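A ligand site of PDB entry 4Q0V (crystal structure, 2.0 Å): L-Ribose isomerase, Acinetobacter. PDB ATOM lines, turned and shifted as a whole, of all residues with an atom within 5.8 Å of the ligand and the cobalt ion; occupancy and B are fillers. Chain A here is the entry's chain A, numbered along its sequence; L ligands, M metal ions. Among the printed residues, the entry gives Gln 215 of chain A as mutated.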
ATOM      1  N   ILE A  51     -33.302 -23.213  12.921  1.00  0.00           N
ATOM      2  CA  ILE A  51     -33.190 -23.489  14.351  1.00  0.00           C
ATOM      3  C   ILE A  51     -33.736 -22.376  15.242  1.00  0.00           C
ATOM      4  O   ILE A  51     -33.482 -21.191  15.012  1.00  0.00           O
ATOM      5  CB  ILE A  51     -31.707 -23.736  14.727  1.00  0.00           C
ATOM      6  CG1 ILE A  51     -31.100 -24.782  13.789  1.00  0.00           C
ATOM      7  CG2 ILE A  51     -31.592 -24.217  16.180  1.00  0.00           C
ATOM      8  CD1 ILE A  51     -29.583 -24.783  13.785  1.00  0.00           C
ATOM      9  N   PHE A  53     -33.859 -21.746  19.313  1.00  0.00           N
ATOM     10  CA  PHE A  53     -33.328 -22.299  20.555  1.00  0.00           C
ATOM     11  C   PHE A  53     -34.236 -22.219  21.788  1.00  0.00           C
ATOM     12  O   PHE A  53     -33.983 -21.436  22.712  1.00  0.00           O
ATOM     13  CB  PHE A  53     -31.975 -21.650  20.867  1.00  0.00           C
ATOM     14  CG  PHE A  53     -30.938 -21.820  19.772  1.00  0.00           C
ATOM     15  CD1 PHE A  53     -30.884 -20.935  18.704  1.00  0.00           C
ATOM     16  CD2 PHE A  53     -30.033 -22.879  19.806  1.00  0.00           C
ATOM     17  CE1 PHE A  53     -29.934 -21.089  17.681  1.00  0.00           C
ATOM     18  CE2 PHE A  53     -29.083 -23.046  18.800  1.00  0.00           C
ATOM     19  CZ  PHE A  53     -29.027 -22.154  17.739  1.00  0.00           C
ATOM     20  N   MET A  74     -31.727 -19.148  14.199  1.00  0.00           N
ATOM     21  CA  MET A  74     -30.825 -18.997  13.065  1.00  0.00           C
ATOM     22  C   MET A  74     -31.015 -20.132  12.068  1.00  0.00           C
ATOM     23  O   MET A  74     -31.682 -21.116  12.342  1.00  0.00           O
ATOM     24  CB  MET A  74     -29.371 -19.030  13.537  1.00  0.00           C
ATOM     25  CG  MET A  74     -28.927 -20.433  13.978  1.00  0.00           C
ATOM     26  SD  MET A  74     -27.324 -20.428  14.802  1.00  0.00           S
ATOM     27  CE  MET A  74     -26.226 -20.163  13.395  1.00  0.00           C
ATOM     28  N   ILE A  76     -28.914 -22.758   9.398  1.00  0.00           N
ATOM     29  CA  ILE A  76     -27.629 -23.370   9.118  1.00  0.00           C
ATOM     30  C   ILE A  76     -27.814 -24.402   8.021  1.00  0.00           C
ATOM     31  O   ILE A  76     -28.666 -25.287   8.122  1.00  0.00           O
ATOM     32  CB  ILE A  76     -27.038 -24.082  10.347  1.00  0.00           C
ATOM     33  CG1 ILE A  76     -26.684 -23.057  11.439  1.00  0.00           C
ATOM     34  CG2 ILE A  76     -25.814 -24.888   9.938  1.00  0.00           C
ATOM     35  CD1 ILE A  76     -26.101 -23.676  12.706  1.00  0.00           C
ATOM     36  N   LYS A 104     -20.407 -25.158   6.812  1.00  0.00           N
ATOM     37  CA  LYS A 104     -21.802 -24.753   6.935  1.00  0.00           C
ATOM     38  C   LYS A 104     -21.970 -23.271   6.666  1.00  0.00           C
ATOM     39  O   LYS A 104     -21.067 -22.477   6.909  1.00  0.00           O
ATOM     40  CB  LYS A 104     -22.300 -25.023   8.364  1.00  0.00           C
ATOM     41  CG  LYS A 104     -21.981 -26.406   8.873  1.00  0.00           C
ATOM     42  CD  LYS A 104     -21.813 -26.427  10.390  1.00  0.00           C
ATOM     43  CE  LYS A 104     -23.127 -26.668  11.112  1.00  0.00           C
ATOM     44  NZ  LYS A 104     -22.873 -27.047  12.535  1.00  0.00           N
ATOM     45  N   MET A 106     -24.174 -20.047   7.713  1.00  0.00           N
ATOM     46  CA  MET A 106     -25.051 -19.623   8.796  1.00  0.00           C
ATOM     47  C   MET A 106     -25.710 -18.306   8.433  1.00  0.00           C
ATOM     48  O   MET A 106     -25.059 -17.372   7.961  1.00  0.00           O
ATOM     49  CB  MET A 106     -24.255 -19.477  10.101  1.00  0.00           C
ATOM     50  CG  MET A 106     -23.457 -20.711  10.476  1.00  0.00           C
ATOM     51  SD  MET A 106     -22.638 -20.596  12.080  1.00  0.00           S
ATOM     52  CE  MET A 106     -21.485 -19.239  11.773  1.00  0.00           C
ATOM     53  N   CYS A 114     -27.048 -16.433  17.845  1.00  0.00           N
ATOM     54  CA  CYS A 114     -26.683 -17.835  17.883  1.00  0.00           C
ATOM     55  C   CYS A 114     -26.309 -17.690  19.376  1.00  0.00           C
ATOM     56  O   CYS A 114     -25.360 -16.975  19.713  1.00  0.00           O
ATOM     57  CB  CYS A 114     -25.432 -18.134  17.069  1.00  0.00           C
ATOM     58  SG  CYS A 114     -24.847 -19.816  17.323  1.00  0.00           S
ATOM     59  N   HIS A 117     -22.703 -20.711  24.050  1.00  0.00           N
ATOM     60  CA  HIS A 117     -22.452 -22.142  24.147  1.00  0.00           C
ATOM     61  C   HIS A 117     -20.981 -22.396  23.912  1.00  0.00           C
ATOM     62  O   HIS A 117     -20.241 -21.488  23.515  1.00  0.00           O
ATOM     63  CB  HIS A 117     -23.262 -22.905  23.094  1.00  0.00           C
ATOM     64  CG  HIS A 117     -22.797 -22.665  21.685  1.00  0.00           C
ATOM     65  ND1 HIS A 117     -23.153 -21.548  20.958  1.00  0.00           N
ATOM     66  CD2 HIS A 117     -21.961 -23.375  20.884  1.00  0.00           C
ATOM     67  CE1 HIS A 117     -22.564 -21.574  19.778  1.00  0.00           C
ATOM     68  NE2 HIS A 117     -21.831 -22.672  19.707  1.00  0.00           N
ATOM     69  N   HIS A 119     -18.017 -25.825  22.862  1.00  0.00           N
ATOM     70  CA  HIS A 119     -17.836 -27.183  22.375  1.00  0.00           C
ATOM     71  C   HIS A 119     -16.608 -27.760  23.058  1.00  0.00           C
ATOM     72  O   HIS A 119     -15.613 -27.067  23.249  1.00  0.00           O
ATOM     73  CB  HIS A 119     -17.599 -27.171  20.860  1.00  0.00           C
ATOM     74  CG  HIS A 119     -18.659 -26.441  20.087  1.00  0.00           C
ATOM     75  ND1 HIS A 119     -19.922 -26.950  19.909  1.00  0.00           N
ATOM     76  CD2 HIS A 119     -18.637 -25.246  19.467  1.00  0.00           C
ATOM     77  CE1 HIS A 119     -20.641 -26.097  19.203  1.00  0.00           C
ATOM     78  NE2 HIS A 119     -19.879 -25.049  18.920  1.00  0.00           N
ATOM     79  N   LYS A 122     -15.037 -29.519  19.201  1.00  0.00           N
ATOM     80  CA  LYS A 122     -15.019 -28.713  17.981  1.00  0.00           C
ATOM     81  C   LYS A 122     -14.437 -27.300  18.013  1.00  0.00           C
ATOM     82  O   LYS A 122     -14.833 -26.468  18.833  1.00  0.00           O
ATOM     83  CB  LYS A 122     -16.427 -28.645  17.390  1.00  0.00           C
ATOM     84  CG  LYS A 122     -16.503 -27.901  16.057  1.00  0.00           C
ATOM     85  CD  LYS A 122     -17.937 -27.840  15.523  1.00  0.00           C
ATOM     86  CE  LYS A 122     -18.811 -26.919  16.360  1.00  0.00           C
ATOM     87  NZ  LYS A 122     -20.181 -26.748  15.789  1.00  0.00           N
ATOM     88  N   GLU A 124     -13.934 -23.928  15.705  1.00  0.00           N
ATOM     89  CA  GLU A 124     -14.617 -23.226  14.618  1.00  0.00           C
ATOM     90  C   GLU A 124     -13.809 -22.071  14.041  1.00  0.00           C
ATOM     91  O   GLU A 124     -12.859 -21.601  14.657  1.00  0.00           O
ATOM     92  CB  GLU A 124     -15.910 -22.593  15.128  1.00  0.00           C
ATOM     93  CG  GLU A 124     -16.981 -23.544  15.487  1.00  0.00           C
ATOM     94  CD  GLU A 124     -18.090 -22.864  16.289  1.00  0.00           C
ATOM     95  OE1 GLU A 124     -18.338 -21.654  16.152  1.00  0.00           O
ATOM     96  OE2 GLU A 124     -18.728 -23.581  17.053  1.00  0.00           O
ATOM     97  N   TYR A 126     -14.649 -18.432  11.383  1.00  0.00           N
ATOM     98  CA  TYR A 126     -15.689 -17.654  10.709  1.00  0.00           C
ATOM     99  C   TYR A 126     -15.193 -16.821   9.544  1.00  0.00           C
ATOM    100  O   TYR A 126     -14.133 -16.191   9.599  1.00  0.00           O
ATOM    101  CB  TYR A 126     -16.377 -16.698  11.699  1.00  0.00           C
ATOM    102  CG  TYR A 126     -16.770 -17.304  13.032  1.00  0.00           C
ATOM    103  CD1 TYR A 126     -17.568 -18.434  13.098  1.00  0.00           C
ATOM    104  CD2 TYR A 126     -16.319 -16.737  14.220  1.00  0.00           C
ATOM    105  CE1 TYR A 126     -17.926 -18.990  14.334  1.00  0.00           C
ATOM    106  CE2 TYR A 126     -16.657 -17.285  15.453  1.00  0.00           C
ATOM    107  CZ  TYR A 126     -17.462 -18.415  15.507  1.00  0.00           C
ATOM    108  OH  TYR A 126     -17.765 -18.975  16.720  1.00  0.00           O
ATOM    109  N   HIS A 199     -18.893 -18.948  23.279  1.00  0.00           N
ATOM    110  CA  HIS A 199     -19.064 -17.990  22.210  1.00  0.00           C
ATOM    111  C   HIS A 199     -20.523 -17.835  21.803  1.00  0.00           C
ATOM    112  O   HIS A 199     -21.354 -18.706  22.046  1.00  0.00           O
ATOM    113  CB  HIS A 199     -18.240 -18.382  20.976  1.00  0.00           C
ATOM    114  CG  HIS A 199     -18.569 -19.734  20.423  1.00  0.00           C
ATOM    115  ND1 HIS A 199     -18.151 -20.908  21.007  1.00  0.00           N
ATOM    116  CD2 HIS A 199     -19.282 -20.086  19.324  1.00  0.00           C
ATOM    117  CE1 HIS A 199     -18.582 -21.933  20.291  1.00  0.00           C
ATOM    118  NE2 HIS A 199     -19.271 -21.465  19.266  1.00  0.00           N
ATOM    119  N   PHE A 201     -23.011 -15.038  18.901  1.00  0.00           N
ATOM    120  CA  PHE A 201     -22.935 -13.985  17.913  1.00  0.00           C
ATOM    121  C   PHE A 201     -24.315 -13.563  17.433  1.00  0.00           C
ATOM    122  O   PHE A 201     -25.292 -14.286  17.575  1.00  0.00           O
ATOM    123  CB  PHE A 201     -22.031 -14.411  16.735  1.00  0.00           C
ATOM    124  CG  PHE A 201     -22.451 -15.676  16.031  1.00  0.00           C
ATOM    125  CD1 PHE A 201     -23.302 -15.635  14.936  1.00  0.00           C
ATOM    126  CD2 PHE A 201     -21.949 -16.913  16.451  1.00  0.00           C
ATOM    127  CE1 PHE A 201     -23.644 -16.816  14.256  1.00  0.00           C
ATOM    128  CE2 PHE A 201     -22.289 -18.085  15.777  1.00  0.00           C
ATOM    129  CZ  PHE A 201     -23.128 -18.036  14.683  1.00  0.00           C
ATOM    130  N   GLN A 215     -18.954 -21.126   8.055  1.00  0.00           N
ATOM    131  CA  GLN A 215     -18.230 -21.717   9.167  1.00  0.00           C
ATOM    132  C   GLN A 215     -17.481 -22.975   8.719  1.00  0.00           C
ATOM    133  O   GLN A 215     -18.080 -23.890   8.145  1.00  0.00           O
ATOM    134  CB  GLN A 215     -19.178 -22.099  10.297  1.00  0.00           C
ATOM    135  CG  GLN A 215     -18.474 -22.616  11.545  1.00  0.00           C
ATOM    136  CD  GLN A 215     -19.391 -23.443  12.433  1.00  0.00           C
ATOM    137  OE1 GLN A 215     -20.516 -23.046  12.706  1.00  0.00           O
ATOM    138  NE2 GLN A 215     -18.904 -24.588  12.878  1.00  0.00           N
ATOM    139  N   SER A 217     -15.187 -25.881  10.350  1.00  0.00           N
ATOM    140  CA  SER A 217     -14.799 -26.387  11.652  1.00  0.00           C
ATOM    141  C   SER A 217     -14.465 -27.859  11.607  1.00  0.00           C
ATOM    142  O   SER A 217     -14.574 -28.499  10.566  1.00  0.00           O
ATOM    143  CB  SER A 217     -15.954 -26.195  12.623  1.00  0.00           C
ATOM    144  OG  SER A 217     -17.001 -27.096  12.315  1.00  0.00           O
ATOM    145  N   SER A 220     -18.844 -31.919  13.450  1.00  0.00           N
ATOM    146  CA  SER A 220     -19.951 -31.416  14.256  1.00  0.00           C
ATOM    147  C   SER A 220     -20.807 -32.570  14.788  1.00  0.00           C
ATOM    148  O   SER A 220     -21.591 -33.164  14.064  1.00  0.00           O
ATOM    149  CB  SER A 220     -20.800 -30.458  13.412  1.00  0.00           C
ATOM    150  OG  SER A 220     -21.905 -29.972  14.138  1.00  0.00           O
ATOM    151  N   GLU A 222     -23.737 -33.501  16.356  1.00  0.00           N
ATOM    152  CA  GLU A 222     -25.047 -32.946  16.687  1.00  0.00           C
ATOM    153  C   GLU A 222     -26.201 -33.872  16.311  1.00  0.00           C
ATOM    154  O   GLU A 222     -26.681 -33.837  15.179  1.00  0.00           O
ATOM    155  CB  GLU A 222     -25.229 -31.601  15.990  1.00  0.00           C
ATOM    156  CG  GLU A 222     -24.150 -30.570  16.287  1.00  0.00           C
ATOM    157  CD  GLU A 222     -24.386 -29.244  15.573  1.00  0.00           C
ATOM    158  OE1 GLU A 222     -24.369 -29.235  14.320  1.00  0.00           O
ATOM    159  OE2 GLU A 222     -24.615 -28.225  16.261  1.00  0.00           O
ATOM    160  N   ASN A 243     -22.405 -30.022  21.943  1.00  0.00           N
ATOM    161  CA  ASN A 243     -22.869 -28.655  22.134  1.00  0.00           C
ATOM    162  C   ASN A 243     -23.315 -28.446  23.568  1.00  0.00           C
ATOM    163  O   ASN A 243     -24.185 -29.155  24.064  1.00  0.00           O
ATOM    164  CB  ASN A 243     -24.016 -28.322  21.181  1.00  0.00           C
ATOM    165  CG  ASN A 243     -23.660 -28.561  19.726  1.00  0.00           C
ATOM    166  OD1 ASN A 243     -22.513 -28.379  19.313  1.00  0.00           O
ATOM    167  ND2 ASN A 243     -24.652 -28.948  18.923  1.00  0.00           N
ATOM    168  N   PHE A 245     -24.864 -25.495  25.644  1.00  0.00           N
ATOM    169  CA  PHE A 245     -25.420 -24.155  25.709  1.00  0.00           C
ATOM    170  C   PHE A 245     -25.559 -23.706  27.164  1.00  0.00           C
ATOM    171  O   PHE A 245     -26.010 -24.467  28.030  1.00  0.00           O
ATOM    172  CB  PHE A 245     -26.780 -24.129  25.015  1.00  0.00           C
ATOM    173  CG  PHE A 245     -26.699 -24.243  23.516  1.00  0.00           C
ATOM    174  CD1 PHE A 245     -26.552 -23.107  22.725  1.00  0.00           C
ATOM    175  CD2 PHE A 245     -26.737 -25.495  22.899  1.00  0.00           C
ATOM    176  CE1 PHE A 245     -26.442 -23.216  21.340  1.00  0.00           C
ATOM    177  CE2 PHE A 245     -26.629 -25.611  21.508  1.00  0.00           C
ATOM    178  CZ  PHE A 245     -26.488 -24.468  20.727  1.00  0.00           C
ATOM    179  N   ARG A 254     -32.452 -26.962  20.310  1.00  0.00           N
ATOM    180  CA  ARG A 254     -31.411 -26.987  19.299  1.00  0.00           C
ATOM    181  C   ARG A 254     -31.606 -28.171  18.350  1.00  0.00           C
ATOM    182  O   ARG A 254     -31.452 -28.029  17.131  1.00  0.00           O
ATOM    183  CB  ARG A 254     -30.036 -27.105  19.968  1.00  0.00           C
ATOM    184  CG  ARG A 254     -28.856 -26.645  19.117  1.00  0.00           C
ATOM    185  CD  ARG A 254     -28.739 -27.403  17.812  1.00  0.00           C
ATOM    186  NE  ARG A 254     -27.676 -26.874  16.964  1.00  0.00           N
ATOM    187  CZ  ARG A 254     -27.498 -27.228  15.690  1.00  0.00           C
ATOM    188  NH1 ARG A 254     -26.500 -26.700  14.992  1.00  0.00           N
ATOM    189  NH2 ARG A 254     -28.333 -28.077  15.113  1.00  0.00           N
HETATM  190  C1  LIG L   1     -21.843 -21.855  15.952  1.00  0.00           C
HETATM  191  O1  LIG L   1     -20.951 -21.504  17.001  1.00  0.00           O
HETATM  192  C2  LIG L   1     -21.946 -23.372  15.840  1.00  0.00           C
HETATM  193  O2  LIG L   1     -21.301 -24.102  16.593  1.00  0.00           O
HETATM  194  C3  LIG L   1     -22.798 -23.984  14.749  1.00  0.00           C
HETATM  195  O3  LIG L   1     -21.981 -24.747  13.890  1.00  0.00           O
HETATM  196  C4  LIG L   1     -23.875 -24.884  15.367  1.00  0.00           C
HETATM  197  O4  LIG L   1     -23.277 -25.931  16.124  1.00  0.00           O
HETATM  198  C5  LIG L   1     -24.795 -24.065  16.255  1.00  0.00           C
HETATM  199  O5  LIG L   1     -25.804 -24.905  16.797  1.00  0.00           O
HETATM  200 CO    CO M   1     -20.218 -23.078  18.179  1.00  0.00          CO
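An oxygen (O3) of the ligand sits at hydrogen-bond distance from the side-chain amide oxygen of Gln 215 (2.5 Å).
An oxygen (O5) of the ligand is in hydrogen-bond range of the guanidinium group of Arg 254 (2.6 Å).
O4 of the ligand is in hydrogen-bond range of OE2 of Glu 222.
The side-chain amino group (NZ) of Lys 104 sits at hydrogen-bond distance from an oxygen (O3) of the ligand, at 2.8 Å.
NZ of Lys 122 sits at hydrogen-bond distance from O4 of the ligand.
NZ of Lys 122 lies close to OE2 of Glu 124.
OE1 of Glu 124 is in hydrogen-bond range of OH of Tyr 126.
A ring nitrogen (ND1) of His 119 lies close to the side-chain amide oxygen of Asn 243 (3.0 Å).
The backbone NH of Gln 215 sits at hydrogen-bond distance from the backbone carbonyl oxygen of Lys 104 (2.8 Å).
The side-chain amide oxygen of Gln 215 lies close to the side-chain sulfur of Met 106 (3.3 Å).
OG of Ser 217 lies within hydrogen-bond range of NE2 of Gln 215, 3.2 Å away.
The side-chain carboxylate of Glu 222 lies within hydrogen-bond range of the side-chain hydroxyl of Ser 220, at 2.6 Å.
SD of Met 74 sits at hydrogen-bond distance from SG of Cys 114 (3.6 Å).
CD1 of Ile 76 touches C4 of the ligand, 3.7 Å away.
Cys 114 touches the ligand (SG to C1, 3.9 Å).
CE2 of Phe 201 touches C1 of the ligand, 3.8 Å away.
Of the 21 residues printed, 12 come within 4 Å of the ligand.
Along chain A the residues within 4 Å of the ligand span positions 76 to 254.
The nearest printed residue that does not touch the ligand is Phe 245 (4.01 Å).
Along chain A the residues within 4 Å of the cobalt ion span positions 117 to 199.
The cobalt ion is bound by OE2 of Glu 124 (1.9 Å), O1 of the ligand (2.1 Å), NE2 of His 119 (2.1 Å), NE2 of His 199 (2.2 Å), O2 of the ligand (2.2 Å) and NE2 of His 117 (2.3 Å).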
